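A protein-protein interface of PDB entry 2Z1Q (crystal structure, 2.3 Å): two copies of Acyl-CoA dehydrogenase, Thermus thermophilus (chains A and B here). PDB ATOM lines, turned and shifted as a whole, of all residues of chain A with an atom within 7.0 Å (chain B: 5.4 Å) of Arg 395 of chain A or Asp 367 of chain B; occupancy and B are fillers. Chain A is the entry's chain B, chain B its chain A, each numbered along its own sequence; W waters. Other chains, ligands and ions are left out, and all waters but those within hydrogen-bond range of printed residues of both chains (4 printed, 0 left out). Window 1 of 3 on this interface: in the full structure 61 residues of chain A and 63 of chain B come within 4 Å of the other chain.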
ATOM      1  N   LEU A 267      25.635 -14.575 -20.681  1.00  0.00           N
ATOM      2  CA  LEU A 267      25.063 -15.900 -20.495  1.00  0.00           C
ATOM      3  C   LEU A 267      23.623 -15.898 -21.031  1.00  0.00           C
ATOM      4  O   LEU A 267      23.176 -16.858 -21.677  1.00  0.00           O
ATOM      5  CB  LEU A 267      25.073 -16.267 -19.006  1.00  0.00           C
ATOM      6  CG  LEU A 267      24.471 -17.625 -18.664  1.00  0.00           C
ATOM      7  CD1 LEU A 267      25.249 -18.703 -19.381  1.00  0.00           C
ATOM      8  CD2 LEU A 267      24.516 -17.848 -17.171  1.00  0.00           C
ATOM      9  N   LYS A 355      19.369 -12.958 -17.343  1.00  0.00           N
ATOM     10  CA  LYS A 355      20.157 -14.126 -16.943  1.00  0.00           C
ATOM     11  C   LYS A 355      19.192 -15.246 -16.516  1.00  0.00           C
ATOM     12  O   LYS A 355      19.334 -16.399 -16.923  1.00  0.00           O
ATOM     13  CB  LYS A 355      21.124 -13.741 -15.805  1.00  0.00           C
ATOM     14  CG  LYS A 355      21.465 -14.866 -14.823  1.00  0.00           C
ATOM     15  CD  LYS A 355      22.255 -15.964 -15.468  1.00  0.00           C
ATOM     16  CE  LYS A 355      21.835 -17.359 -14.968  1.00  0.00           C
ATOM     17  NZ  LYS A 355      22.061 -17.617 -13.522  1.00  0.00           N
ATOM     18  N   VAL A 356      18.188 -14.888 -15.726  1.00  0.00           N
ATOM     19  CA  VAL A 356      17.178 -15.830 -15.256  1.00  0.00           C
ATOM     20  C   VAL A 356      16.258 -16.233 -16.400  1.00  0.00           C
ATOM     21  O   VAL A 356      15.946 -17.409 -16.564  1.00  0.00           O
ATOM     22  CB  VAL A 356      16.312 -15.210 -14.150  1.00  0.00           C
ATOM     23  CG1 VAL A 356      15.284 -16.229 -13.655  1.00  0.00           C
ATOM     24  CG2 VAL A 356      17.192 -14.734 -13.017  1.00  0.00           C
ATOM     25  N   SER A 359      18.294 -18.557 -19.210  1.00  0.00           N
ATOM     26  CA  SER A 359      18.510 -19.922 -18.768  1.00  0.00           C
ATOM     27  C   SER A 359      17.205 -20.707 -18.645  1.00  0.00           C
ATOM     28  O   SER A 359      17.161 -21.865 -19.040  1.00  0.00           O
ATOM     29  CB  SER A 359      19.290 -19.936 -17.441  1.00  0.00           C
ATOM     30  OG  SER A 359      18.749 -19.029 -16.497  1.00  0.00           O
ATOM     31  N   GLU A 360      16.135 -20.086 -18.139  1.00  0.00           N
ATOM     32  CA  GLU A 360      14.869 -20.810 -17.986  1.00  0.00           C
ATOM     33  C   GLU A 360      14.174 -21.074 -19.305  1.00  0.00           C
ATOM     34  O   GLU A 360      13.480 -22.083 -19.454  1.00  0.00           O
ATOM     35  CB  GLU A 360      13.952 -20.080 -17.004  1.00  0.00           C
ATOM     36  CG  GLU A 360      14.570 -20.118 -15.603  1.00  0.00           C
ATOM     37  CD  GLU A 360      13.665 -19.592 -14.505  1.00  0.00           C
ATOM     38  OE1 GLU A 360      14.125 -19.589 -13.345  1.00  0.00           O
ATOM     39  OE2 GLU A 360      12.507 -19.189 -14.780  1.00  0.00           O
ATOM     40  N   ASP A 363      16.154 -23.956 -20.826  1.00  0.00           N
ATOM     41  CA  ASP A 363      15.787 -25.163 -20.084  1.00  0.00           C
ATOM     42  C   ASP A 363      14.537 -25.773 -20.724  1.00  0.00           C
ATOM     43  O   ASP A 363      14.508 -26.959 -21.082  1.00  0.00           O
ATOM     44  CB  ASP A 363      15.520 -24.777 -18.619  1.00  0.00           C
ATOM     45  CG  ASP A 363      15.139 -25.963 -17.737  1.00  0.00           C
ATOM     46  OD1 ASP A 363      16.027 -26.546 -17.067  1.00  0.00           O
ATOM     47  OD2 ASP A 363      13.943 -26.315 -17.719  1.00  0.00           O
ATOM     48  N   TYR A 388      20.567 -30.981 -23.733  1.00  0.00           N
ATOM     49  CA  TYR A 388      19.753 -31.089 -22.531  1.00  0.00           C
ATOM     50  C   TYR A 388      20.697 -31.091 -21.330  1.00  0.00           C
ATOM     51  O   TYR A 388      20.449 -30.403 -20.335  1.00  0.00           O
ATOM     52  CB  TYR A 388      18.960 -32.390 -22.539  1.00  0.00           C
ATOM     53  CG  TYR A 388      18.081 -32.581 -21.319  1.00  0.00           C
ATOM     54  CD1 TYR A 388      16.839 -31.959 -21.240  1.00  0.00           C
ATOM     55  CD2 TYR A 388      18.494 -33.380 -20.245  1.00  0.00           C
ATOM     56  CE1 TYR A 388      16.022 -32.122 -20.132  1.00  0.00           C
ATOM     57  CE2 TYR A 388      17.674 -33.550 -19.125  1.00  0.00           C
ATOM     58  CZ  TYR A 388      16.437 -32.913 -19.085  1.00  0.00           C
ATOM     59  OH  TYR A 388      15.579 -33.048 -18.023  1.00  0.00           O
ATOM     60  N   ALA A 391      22.694 -27.642 -20.885  1.00  0.00           N
ATOM     61  CA  ALA A 391      21.850 -26.535 -20.441  1.00  0.00           C
ATOM     62  C   ALA A 391      21.691 -26.400 -18.941  1.00  0.00           C
ATOM     63  O   ALA A 391      21.682 -25.295 -18.405  1.00  0.00           O
ATOM     64  CB  ALA A 391      20.482 -26.653 -21.075  1.00  0.00           C
ATOM     65  N   ARG A 392      21.557 -27.544 -18.285  1.00  0.00           N
ATOM     66  CA  ARG A 392      21.334 -27.619 -16.845  1.00  0.00           C
ATOM     67  C   ARG A 392      22.213 -26.698 -15.972  1.00  0.00           C
ATOM     68  O   ARG A 392      21.733 -26.126 -14.984  1.00  0.00           O
ATOM     69  CB  ARG A 392      21.489 -29.084 -16.390  1.00  0.00           C
ATOM     70  CG  ARG A 392      20.461 -29.533 -15.357  1.00  0.00           C
ATOM     71  CD  ARG A 392      20.314 -28.454 -14.347  1.00  0.00           C
ATOM     72  NE  ARG A 392      19.153 -28.505 -13.481  1.00  0.00           N
ATOM     73  CZ  ARG A 392      18.877 -27.506 -12.654  1.00  0.00           C
ATOM     74  NH1 ARG A 392      17.821 -27.543 -11.849  1.00  0.00           N
ATOM     75  NH2 ARG A 392      19.664 -26.443 -12.668  1.00  0.00           N
ATOM     76  N   ILE A 393      23.484 -26.541 -16.328  1.00  0.00           N
ATOM     77  CA  ILE A 393      24.389 -25.708 -15.532  1.00  0.00           C
ATOM     78  C   ILE A 393      24.032 -24.217 -15.517  1.00  0.00           C
ATOM     79  O   ILE A 393      24.314 -23.508 -14.550  1.00  0.00           O
ATOM     80  CB  ILE A 393      25.856 -25.879 -16.027  1.00  0.00           C
ATOM     81  CG1 ILE A 393      26.834 -25.293 -15.003  1.00  0.00           C
ATOM     82  CG2 ILE A 393      26.039 -25.201 -17.382  1.00  0.00           C
ATOM     83  CD1 ILE A 393      26.749 -25.938 -13.623  1.00  0.00           C
ATOM     84  N   ASN A 394      23.374 -23.745 -16.565  1.00  0.00           N
ATOM     85  CA  ASN A 394      23.030 -22.333 -16.659  1.00  0.00           C
ATOM     86  C   ASN A 394      22.230 -21.673 -15.550  1.00  0.00           C
ATOM     87  O   ASN A 394      22.471 -20.510 -15.243  1.00  0.00           O
ATOM     88  CB  ASN A 394      22.400 -22.076 -18.017  1.00  0.00           C
ATOM     89  CG  ASN A 394      23.390 -22.314 -19.124  1.00  0.00           C
ATOM     90  OD1 ASN A 394      24.487 -21.753 -19.105  1.00  0.00           O
ATOM     91  ND2 ASN A 394      23.034 -23.162 -20.077  1.00  0.00           N
ATOM     92  N   ARG A 395      21.307 -22.404 -14.936  1.00  0.00           N
ATOM     93  CA  ARG A 395      20.508 -21.857 -13.841  1.00  0.00           C
ATOM     94  C   ARG A 395      21.338 -21.753 -12.558  1.00  0.00           C
ATOM     95  O   ARG A 395      20.850 -21.289 -11.522  1.00  0.00           O
ATOM     96  CB  ARG A 395      19.275 -22.733 -13.614  1.00  0.00           C
ATOM     97  CG  ARG A 395      18.258 -22.670 -14.758  1.00  0.00           C
ATOM     98  CD  ARG A 395      17.469 -23.982 -14.867  1.00  0.00           C
ATOM     99  NE  ARG A 395      16.668 -24.268 -13.678  1.00  0.00           N
ATOM    100  CZ  ARG A 395      16.053 -25.426 -13.453  1.00  0.00           C
ATOM    101  NH1 ARG A 395      16.138 -26.415 -14.323  1.00  0.00           N
ATOM    102  NH2 ARG A 395      15.348 -25.593 -12.342  1.00  0.00           N
ATOM    103  N   ILE A 396      22.594 -22.184 -12.631  1.00  0.00           N
ATOM    104  CA  ILE A 396      23.496 -22.124 -11.477  1.00  0.00           C
ATOM    105  C   ILE A 396      24.592 -21.074 -11.675  1.00  0.00           C
ATOM    106  O   ILE A 396      24.902 -20.319 -10.746  1.00  0.00           O
ATOM    107  CB  ILE A 396      24.107 -23.501 -11.218  1.00  0.00           C
ATOM    108  CG1 ILE A 396      22.971 -24.461 -10.890  1.00  0.00           C
ATOM    109  CG2 ILE A 396      25.124 -23.455 -10.075  1.00  0.00           C
ATOM    110  CD1 ILE A 396      23.410 -25.856 -10.700  1.00  0.00           C
ATOM    111  N   PHE A 397      25.148 -21.020 -12.888  1.00  0.00           N
ATOM    112  CA  PHE A 397      26.186 -20.063 -13.291  1.00  0.00           C
ATOM    113  C   PHE A 397      25.774 -18.603 -13.066  1.00  0.00           C
ATOM    114  O   PHE A 397      24.593 -18.267 -13.102  1.00  0.00           O
ATOM    115  CB  PHE A 397      26.496 -20.189 -14.794  1.00  0.00           C
ATOM    116  CG  PHE A 397      27.477 -21.283 -15.146  1.00  0.00           C
ATOM    117  CD1 PHE A 397      28.310 -21.824 -14.183  1.00  0.00           C
ATOM    118  CD2 PHE A 397      27.600 -21.726 -16.464  1.00  0.00           C
ATOM    119  CE1 PHE A 397      29.254 -22.782 -14.522  1.00  0.00           C
ATOM    120  CE2 PHE A 397      28.546 -22.688 -16.814  1.00  0.00           C
ATOM    121  CZ  PHE A 397      29.375 -23.217 -15.849  1.00  0.00           C
ATOM    122  N   GLU A 398      26.771 -17.741 -12.878  1.00  0.00           N
ATOM    123  CA  GLU A 398      26.543 -16.305 -12.693  1.00  0.00           C
ATOM    124  C   GLU A 398      25.551 -16.049 -11.570  1.00  0.00           C
ATOM    125  O   GLU A 398      24.733 -15.133 -11.654  1.00  0.00           O
ATOM    126  CB  GLU A 398      25.975 -15.687 -13.980  1.00  0.00           C
ATOM    127  CG  GLU A 398      26.681 -16.110 -15.260  1.00  0.00           C
ATOM    128  CD  GLU A 398      28.126 -15.652 -15.310  1.00  0.00           C
ATOM    129  OE1 GLU A 398      28.928 -16.317 -15.999  1.00  0.00           O
ATOM    130  OE2 GLU A 398      28.466 -14.630 -14.674  1.00  0.00           O
ATOM    131  N   GLY A 399      25.630 -16.854 -10.519  1.00  0.00           N
ATOM    132  CA  GLY A 399      24.691 -16.727  -9.422  1.00  0.00           C
ATOM    133  C   GLY A 399      23.510 -17.608  -9.784  1.00  0.00           C
ATOM    134  O   GLY A 399      23.057 -17.601 -10.937  1.00  0.00           O
ATOM    135  N   THR A 400      23.024 -18.385  -8.815  1.00  0.00           N
ATOM    136  CA  THR A 400      21.891 -19.266  -9.048  1.00  0.00           C
ATOM    137  C   THR A 400      20.692 -18.360  -9.321  1.00  0.00           C
ATOM    138  O   THR A 400      20.721 -17.171  -8.984  1.00  0.00           O
ATOM    139  CB  THR A 400      21.569 -20.117  -7.802  1.00  0.00           C
ATOM    140  OG1 THR A 400      21.073 -19.266  -6.762  1.00  0.00           O
ATOM    141  CG2 THR A 400      22.801 -20.835  -7.303  1.00  0.00           C
ATOM    142  N   ASN A 401      19.638 -18.922  -9.908  1.00  0.00           N
ATOM    143  CA  ASN A 401      18.456 -18.125 -10.191  1.00  0.00           C
ATOM    144  C   ASN A 401      17.763 -17.660  -8.913  1.00  0.00           C
ATOM    145  O   ASN A 401      17.036 -16.667  -8.930  1.00  0.00           O
ATOM    146  CB  ASN A 401      17.512 -18.902 -11.102  1.00  0.00           C
ATOM    147  CG  ASN A 401      18.009 -18.930 -12.535  1.00  0.00           C
ATOM    148  OD1 ASN A 401      19.024 -18.306 -12.852  1.00  0.00           O
ATOM    149  ND2 ASN A 401      17.304 -19.634 -13.402  1.00  0.00           N
ATOM    150  N   GLU A 402      17.993 -18.377  -7.809  1.00  0.00           N
ATOM    151  CA  GLU A 402      17.431 -17.987  -6.515  1.00  0.00           C
ATOM    152  C   GLU A 402      18.106 -16.666  -6.120  1.00  0.00           C
ATOM    153  O   GLU A 402      17.436 -15.679  -5.822  1.00  0.00           O
ATOM    154  CB  GLU A 402      17.715 -19.049  -5.439  1.00  0.00           C
ATOM    155  CG  GLU A 402      16.933 -20.362  -5.587  1.00  0.00           C
ATOM    156  CD  GLU A 402      17.334 -21.166  -6.802  1.00  0.00           C
ATOM    157  OE1 GLU A 402      18.512 -21.572  -6.893  1.00  0.00           O
ATOM    158  OE2 GLU A 402      16.474 -21.393  -7.673  1.00  0.00           O
ATOM    159  N   ASN A 404      19.678 -14.511  -7.987  1.00  0.00           N
ATOM    160  CA  ASN A 404      19.300 -13.441  -8.905  1.00  0.00           C
ATOM    161  C   ASN A 404      17.881 -12.949  -8.639  1.00  0.00           C
ATOM    162  O   ASN A 404      17.615 -11.750  -8.721  1.00  0.00           O
ATOM    163  CB  ASN A 404      19.445 -13.914 -10.348  1.00  0.00           C
ATOM    164  CG  ASN A 404      20.872 -13.824 -10.834  1.00  0.00           C
ATOM    165  OD1 ASN A 404      21.391 -12.725 -11.046  1.00  0.00           O
ATOM    166  ND2 ASN A 404      21.525 -14.976 -11.002  1.00  0.00           N
ATOM    167  N   LEU B 362       8.037 -36.410 -10.714  1.00  0.00           N
ATOM    168  CA  LEU B 362       9.436 -36.792 -10.526  1.00  0.00           C
ATOM    169  C   LEU B 362      10.377 -35.881 -11.302  1.00  0.00           C
ATOM    170  O   LEU B 362      11.518 -35.674 -10.893  1.00  0.00           O
ATOM    171  CB  LEU B 362       9.666 -38.250 -10.958  1.00  0.00           C
ATOM    172  CG  LEU B 362      11.117 -38.743 -11.013  1.00  0.00           C
ATOM    173  CD1 LEU B 362      11.772 -38.604  -9.627  1.00  0.00           C
ATOM    174  CD2 LEU B 362      11.146 -40.189 -11.481  1.00  0.00           C
ATOM    175  N   ASP B 363       9.896 -35.340 -12.418  1.00  0.00           N
ATOM    176  CA  ASP B 363      10.698 -34.433 -13.228  1.00  0.00           C
ATOM    177  C   ASP B 363      10.988 -33.175 -12.440  1.00  0.00           C
ATOM    178  O   ASP B 363      12.094 -32.647 -12.485  1.00  0.00           O
ATOM    179  CB  ASP B 363       9.969 -34.020 -14.497  1.00  0.00           C
ATOM    180  CG  ASP B 363       9.751 -35.166 -15.428  1.00  0.00           C
ATOM    181  OD1 ASP B 363      10.697 -35.960 -15.620  1.00  0.00           O
ATOM    182  OD2 ASP B 363       8.634 -35.261 -15.971  1.00  0.00           O
ATOM    183  N   TYR B 364       9.969 -32.675 -11.747  1.00  0.00           N
ATOM    184  CA  TYR B 364      10.124 -31.472 -10.947  1.00  0.00           C
ATOM    185  C   TYR B 364      11.033 -31.797  -9.762  1.00  0.00           C
ATOM    186  O   TYR B 364      11.971 -31.071  -9.473  1.00  0.00           O
ATOM    187  CB  TYR B 364       8.764 -30.979 -10.432  1.00  0.00           C
ATOM    188  CG  TYR B 364       8.838 -29.816  -9.449  1.00  0.00           C
ATOM    189  CD1 TYR B 364       9.118 -28.521  -9.886  1.00  0.00           C
ATOM    190  CD2 TYR B 364       8.666 -30.021  -8.075  1.00  0.00           C
ATOM    191  CE1 TYR B 364       9.232 -27.463  -8.991  1.00  0.00           C
ATOM    192  CE2 TYR B 364       8.781 -28.957  -7.166  1.00  0.00           C
ATOM    193  CZ  TYR B 364       9.066 -27.685  -7.637  1.00  0.00           C
ATOM    194  OH  TYR B 364       9.193 -26.609  -6.785  1.00  0.00           O
ATOM    195  N   VAL B 365      10.750 -32.904  -9.085  1.00  0.00           N
ATOM    196  CA  VAL B 365      11.533 -33.280  -7.914  1.00  0.00           C
ATOM    197  C   VAL B 365      13.040 -33.362  -8.195  1.00  0.00           C
ATOM    198  O   VAL B 365      13.820 -32.712  -7.488  1.00  0.00           O
ATOM    199  CB  VAL B 365      10.985 -34.598  -7.308  1.00  0.00           C
ATOM    200  CG1 VAL B 365      11.763 -34.977  -6.041  1.00  0.00           C
ATOM    201  CG2 VAL B 365       9.514 -34.406  -6.946  1.00  0.00           C
ATOM    202  N   VAL B 366      13.450 -34.120  -9.223  1.00  0.00           N
ATOM    203  CA  VAL B 366      14.881 -34.228  -9.560  1.00  0.00           C
ATOM    204  C   VAL B 366      15.448 -32.897 -10.068  1.00  0.00           C
ATOM    205  O   VAL B 366      16.619 -32.609  -9.856  1.00  0.00           O
ATOM    206  CB  VAL B 366      15.181 -35.336 -10.634  1.00  0.00           C
ATOM    207  CG1 VAL B 366      14.759 -36.709 -10.108  1.00  0.00           C
ATOM    208  CG2 VAL B 366      14.498 -34.996 -11.961  1.00  0.00           C
ATOM    209  N   ASP B 367      14.630 -32.083 -10.729  1.00  0.00           N
ATOM    210  CA  ASP B 367      15.121 -30.802 -11.239  1.00  0.00           C
ATOM    211  C   ASP B 367      15.492 -29.888 -10.090  1.00  0.00           C
ATOM    212  O   ASP B 367      16.606 -29.355 -10.053  1.00  0.00           O
ATOM    213  CB  ASP B 367      14.061 -30.100 -12.111  1.00  0.00           C
ATOM    214  CG  ASP B 367      14.540 -28.743 -12.655  1.00  0.00           C
ATOM    215  OD1 ASP B 367      15.680 -28.677 -13.181  1.00  0.00           O
ATOM    216  OD2 ASP B 367      13.775 -27.753 -12.556  1.00  0.00           O
ATOM    217  N   GLU B 368      14.563 -29.718  -9.151  1.00  0.00           N
ATOM    218  CA  GLU B 368      14.783 -28.854  -7.998  1.00  0.00           C
ATOM    219  C   GLU B 368      15.805 -29.467  -7.052  1.00  0.00           C
ATOM    220  O   GLU B 368      16.483 -28.764  -6.302  1.00  0.00           O
ATOM    221  CB  GLU B 368      13.461 -28.608  -7.254  1.00  0.00           C
ATOM    222  CG  GLU B 368      12.468 -27.754  -8.035  1.00  0.00           C
ATOM    223  CD  GLU B 368      12.991 -26.355  -8.335  1.00  0.00           C
ATOM    224  OE1 GLU B 368      12.294 -25.595  -9.032  1.00  0.00           O
ATOM    225  OE2 GLU B 368      14.103 -26.005  -7.871  1.00  0.00           O
ATOM    226  N   GLY B 369      15.898 -30.790  -7.083  1.00  0.00           N
ATOM    227  CA  GLY B 369      16.871 -31.478  -6.261  1.00  0.00           C
ATOM    228  C   GLY B 369      18.251 -31.024  -6.701  1.00  0.00           C
ATOM    229  O   GLY B 369      19.093 -30.700  -5.857  1.00  0.00           O
ATOM    230  N   VAL B 370      18.486 -30.980  -8.018  1.00  0.00           N
ATOM    231  CA  VAL B 370      19.787 -30.533  -8.531  1.00  0.00           C
ATOM    232  C   VAL B 370      19.991 -29.084  -8.109  1.00  0.00           C
ATOM    233  O   VAL B 370      21.074 -28.710  -7.632  1.00  0.00           O
ATOM    234  CB  VAL B 370      19.864 -30.624 -10.086  1.00  0.00           C
ATOM    235  CG1 VAL B 370      21.170 -29.995 -10.613  1.00  0.00           C
ATOM    236  CG2 VAL B 370      19.794 -32.085 -10.515  1.00  0.00           C
ATOM    237  N   GLN B 371      18.943 -28.274  -8.256  1.00  0.00           N
ATOM    238  CA  GLN B 371      19.034 -26.868  -7.907  1.00  0.00           C
ATOM    239  C   GLN B 371      19.494 -26.664  -6.461  1.00  0.00           C
ATOM    240  O   GLN B 371      20.387 -25.863  -6.217  1.00  0.00           O
ATOM    241  CB  GLN B 371      17.697 -26.162  -8.150  1.00  0.00           C
ATOM    242  CG  GLN B 371      17.812 -24.649  -8.260  1.00  0.00           C
ATOM    243  CD  GLN B 371      18.727 -24.198  -9.402  1.00  0.00           C
ATOM    244  OE1 GLN B 371      18.920 -24.923 -10.381  1.00  0.00           O
ATOM    245  NE2 GLN B 371      19.272 -22.999  -9.289  1.00  0.00           N
ATOM    246  N   TYR B 388      18.638 -37.072 -11.981  1.00  0.00           N
ATOM    247  CA  TYR B 388      18.177 -36.112 -12.997  1.00  0.00           C
ATOM    248  C   TYR B 388      18.242 -36.714 -14.398  1.00  0.00           C
ATOM    249  O   TYR B 388      17.314 -36.559 -15.184  1.00  0.00           O
ATOM    250  CB  TYR B 388      19.038 -34.857 -12.957  1.00  0.00           C
ATOM    251  CG  TYR B 388      18.651 -33.796 -13.963  1.00  0.00           C
ATOM    252  CD1 TYR B 388      17.593 -32.933 -13.705  1.00  0.00           C
ATOM    253  CD2 TYR B 388      19.360 -33.635 -15.161  1.00  0.00           C
ATOM    254  CE1 TYR B 388      17.243 -31.932 -14.599  1.00  0.00           C
ATOM    255  CE2 TYR B 388      19.020 -32.621 -16.070  1.00  0.00           C
ATOM    256  CZ  TYR B 388      17.958 -31.775 -15.778  1.00  0.00           C
ATOM    257  OH  TYR B 388      17.602 -30.755 -16.631  1.00  0.00           O
HETATM  258  O   HOH W   1      15.931 -22.679 -10.164  1.00  0.00           O
HETATM  259  O   HOH W   2      15.417 -34.791 -15.708  1.00  0.00           O
HETATM  260  O   HOH W   3      15.722 -29.090 -15.950  1.00  0.00           O
HETATM  261  O   HOH W   4      18.241 -29.404 -19.203  1.00  0.00           O
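Water W3 lies within hydrogen-bond range of the side-chain hydroxyl of Tyr 388 of chain B, the side-chain carboxylate of Asp 363 of chain A, the side-chain carboxylate of Asp 367 of chain B and the guanidinium group of Arg 395 of chain A. Water W2 lies within hydrogen-bond range of the backbone carbonyl oxygen of Tyr 388 of chain B and the side-chain hydroxyl of Tyr 388 of chain A. Water W4 bridges the backbone carbonyl oxygen (O) of Tyr 388 of chain A and the side-chain hydroxyl (OH) of Tyr 388 of chain B. Water W1 bridges OE2 of Glu 402 of chain A (2.9 Å) and NE2 of Gln 371 of chain B (3.5 Å).
NE of Arg 392 of chain A touches CG1 of Val 370 of chain B (3.8 Å). Tyr 388 of chain B touches Arg 392 of chain A. Gln 371 of chain B touches Thr 400 of chain A (NE2 to CB, 3.97 Å).
Tyr 388 of chain A touches its own counterpart, Tyr 388 of chain B. Positions printed for both chains: 363 and 388. Of the 9 pairs that touch across the chains among the printed residues, 1 has its exchanged pair printed and touching as well.
Printed residues of chain A that touch a printed residue of chain B: Tyr 388, Arg 392, Arg 395, Thr 400 and Glu 402. Hydrophobic or aromatic side chains of chain A within 4 Å of the printed part of chain B: Tyr 388. Printed residues of chain B that touch a printed residue of chain A: Asp 367, Val 370, Gln 371 and Tyr 388. Hydrophobic or aromatic side chains of chain B that line the printed part of chain A: Val 370 and Tyr 388. Among the printed residues, 9 pairs touch across the chains. Among the printed residues, Asp or Glu carboxylates within 4 Å of a Lys or Arg side-chain nitrogen of the other chain: Arg 392 of chain A with Asp 367 of chain B and Arg 395 of chain A with Asp 367 of chain B.
The side-chain carboxylate (OD1) of Asp 367 of chain B lies within salt-bridge range of the guanidinium group (NH1) of Arg 392 of chain A (2.8 Å). OD1 of Asp 367 of chain B lies within salt-bridge range of NH1 of Arg 395 of chain A (2.6 Å). The side-chain amide oxygen (OE1) of Gln 371 of chain B is in hydrogen-bond range of the guanidinium group (NH2) of Arg 392 of chain A (2.8 Å). NE2 of Gln 371 of chain B lies within hydrogen-bond range of O of Arg 395 of chain A (3.2 Å). NE2 of Gln 371 of chain B lies within hydrogen-bond range of OE1 of Glu 402 of chain A. The side-chain hydroxyl (OH) of Tyr 388 of chain B sits at hydrogen-bond distance from the side-chain hydroxyl (OH) of Tyr 388 of chain A.
Arg 395 of chain A touches just these residues of chain B: Asp 367 and Gln 371. Of chain A, only Arg 392 and Arg 395 come within 4 Å of Asp 367 of chain B. Of the printed residues of chain A, Tyr 388 of chain B touches Tyr 388 and Arg 392. Printed residues of chain B within 4 Å of Glu 402 of chain A: Gln 371 (2.9 Å). The nearest residue of chain A that does not touch Asp 367 of chain B is Asp 363 of chain A (4.4 Å). The nearest printed residue of chain B that does not touch Arg 392 of chain A is Glu 368 of chain B (4.8 Å).
OD1 of Asp 363 of chain A is in salt-bridge range of NH1 of Arg 395 of chain A. The backbone carbonyl oxygen (O) of Arg 395 of chain A is in hydrogen-bond range of the backbone NH (N) of Asn 401 of chain A (3.1 Å). The side-chain hydroxyl (OG1) of Thr 400 of chain A lies close to the backbone NH (N) of Glu 402 of chain A, at 3.4 Å. ND2 of Asn 404 of chain A is in hydrogen-bond range of O of Thr 400 of chain A (3.1 Å).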
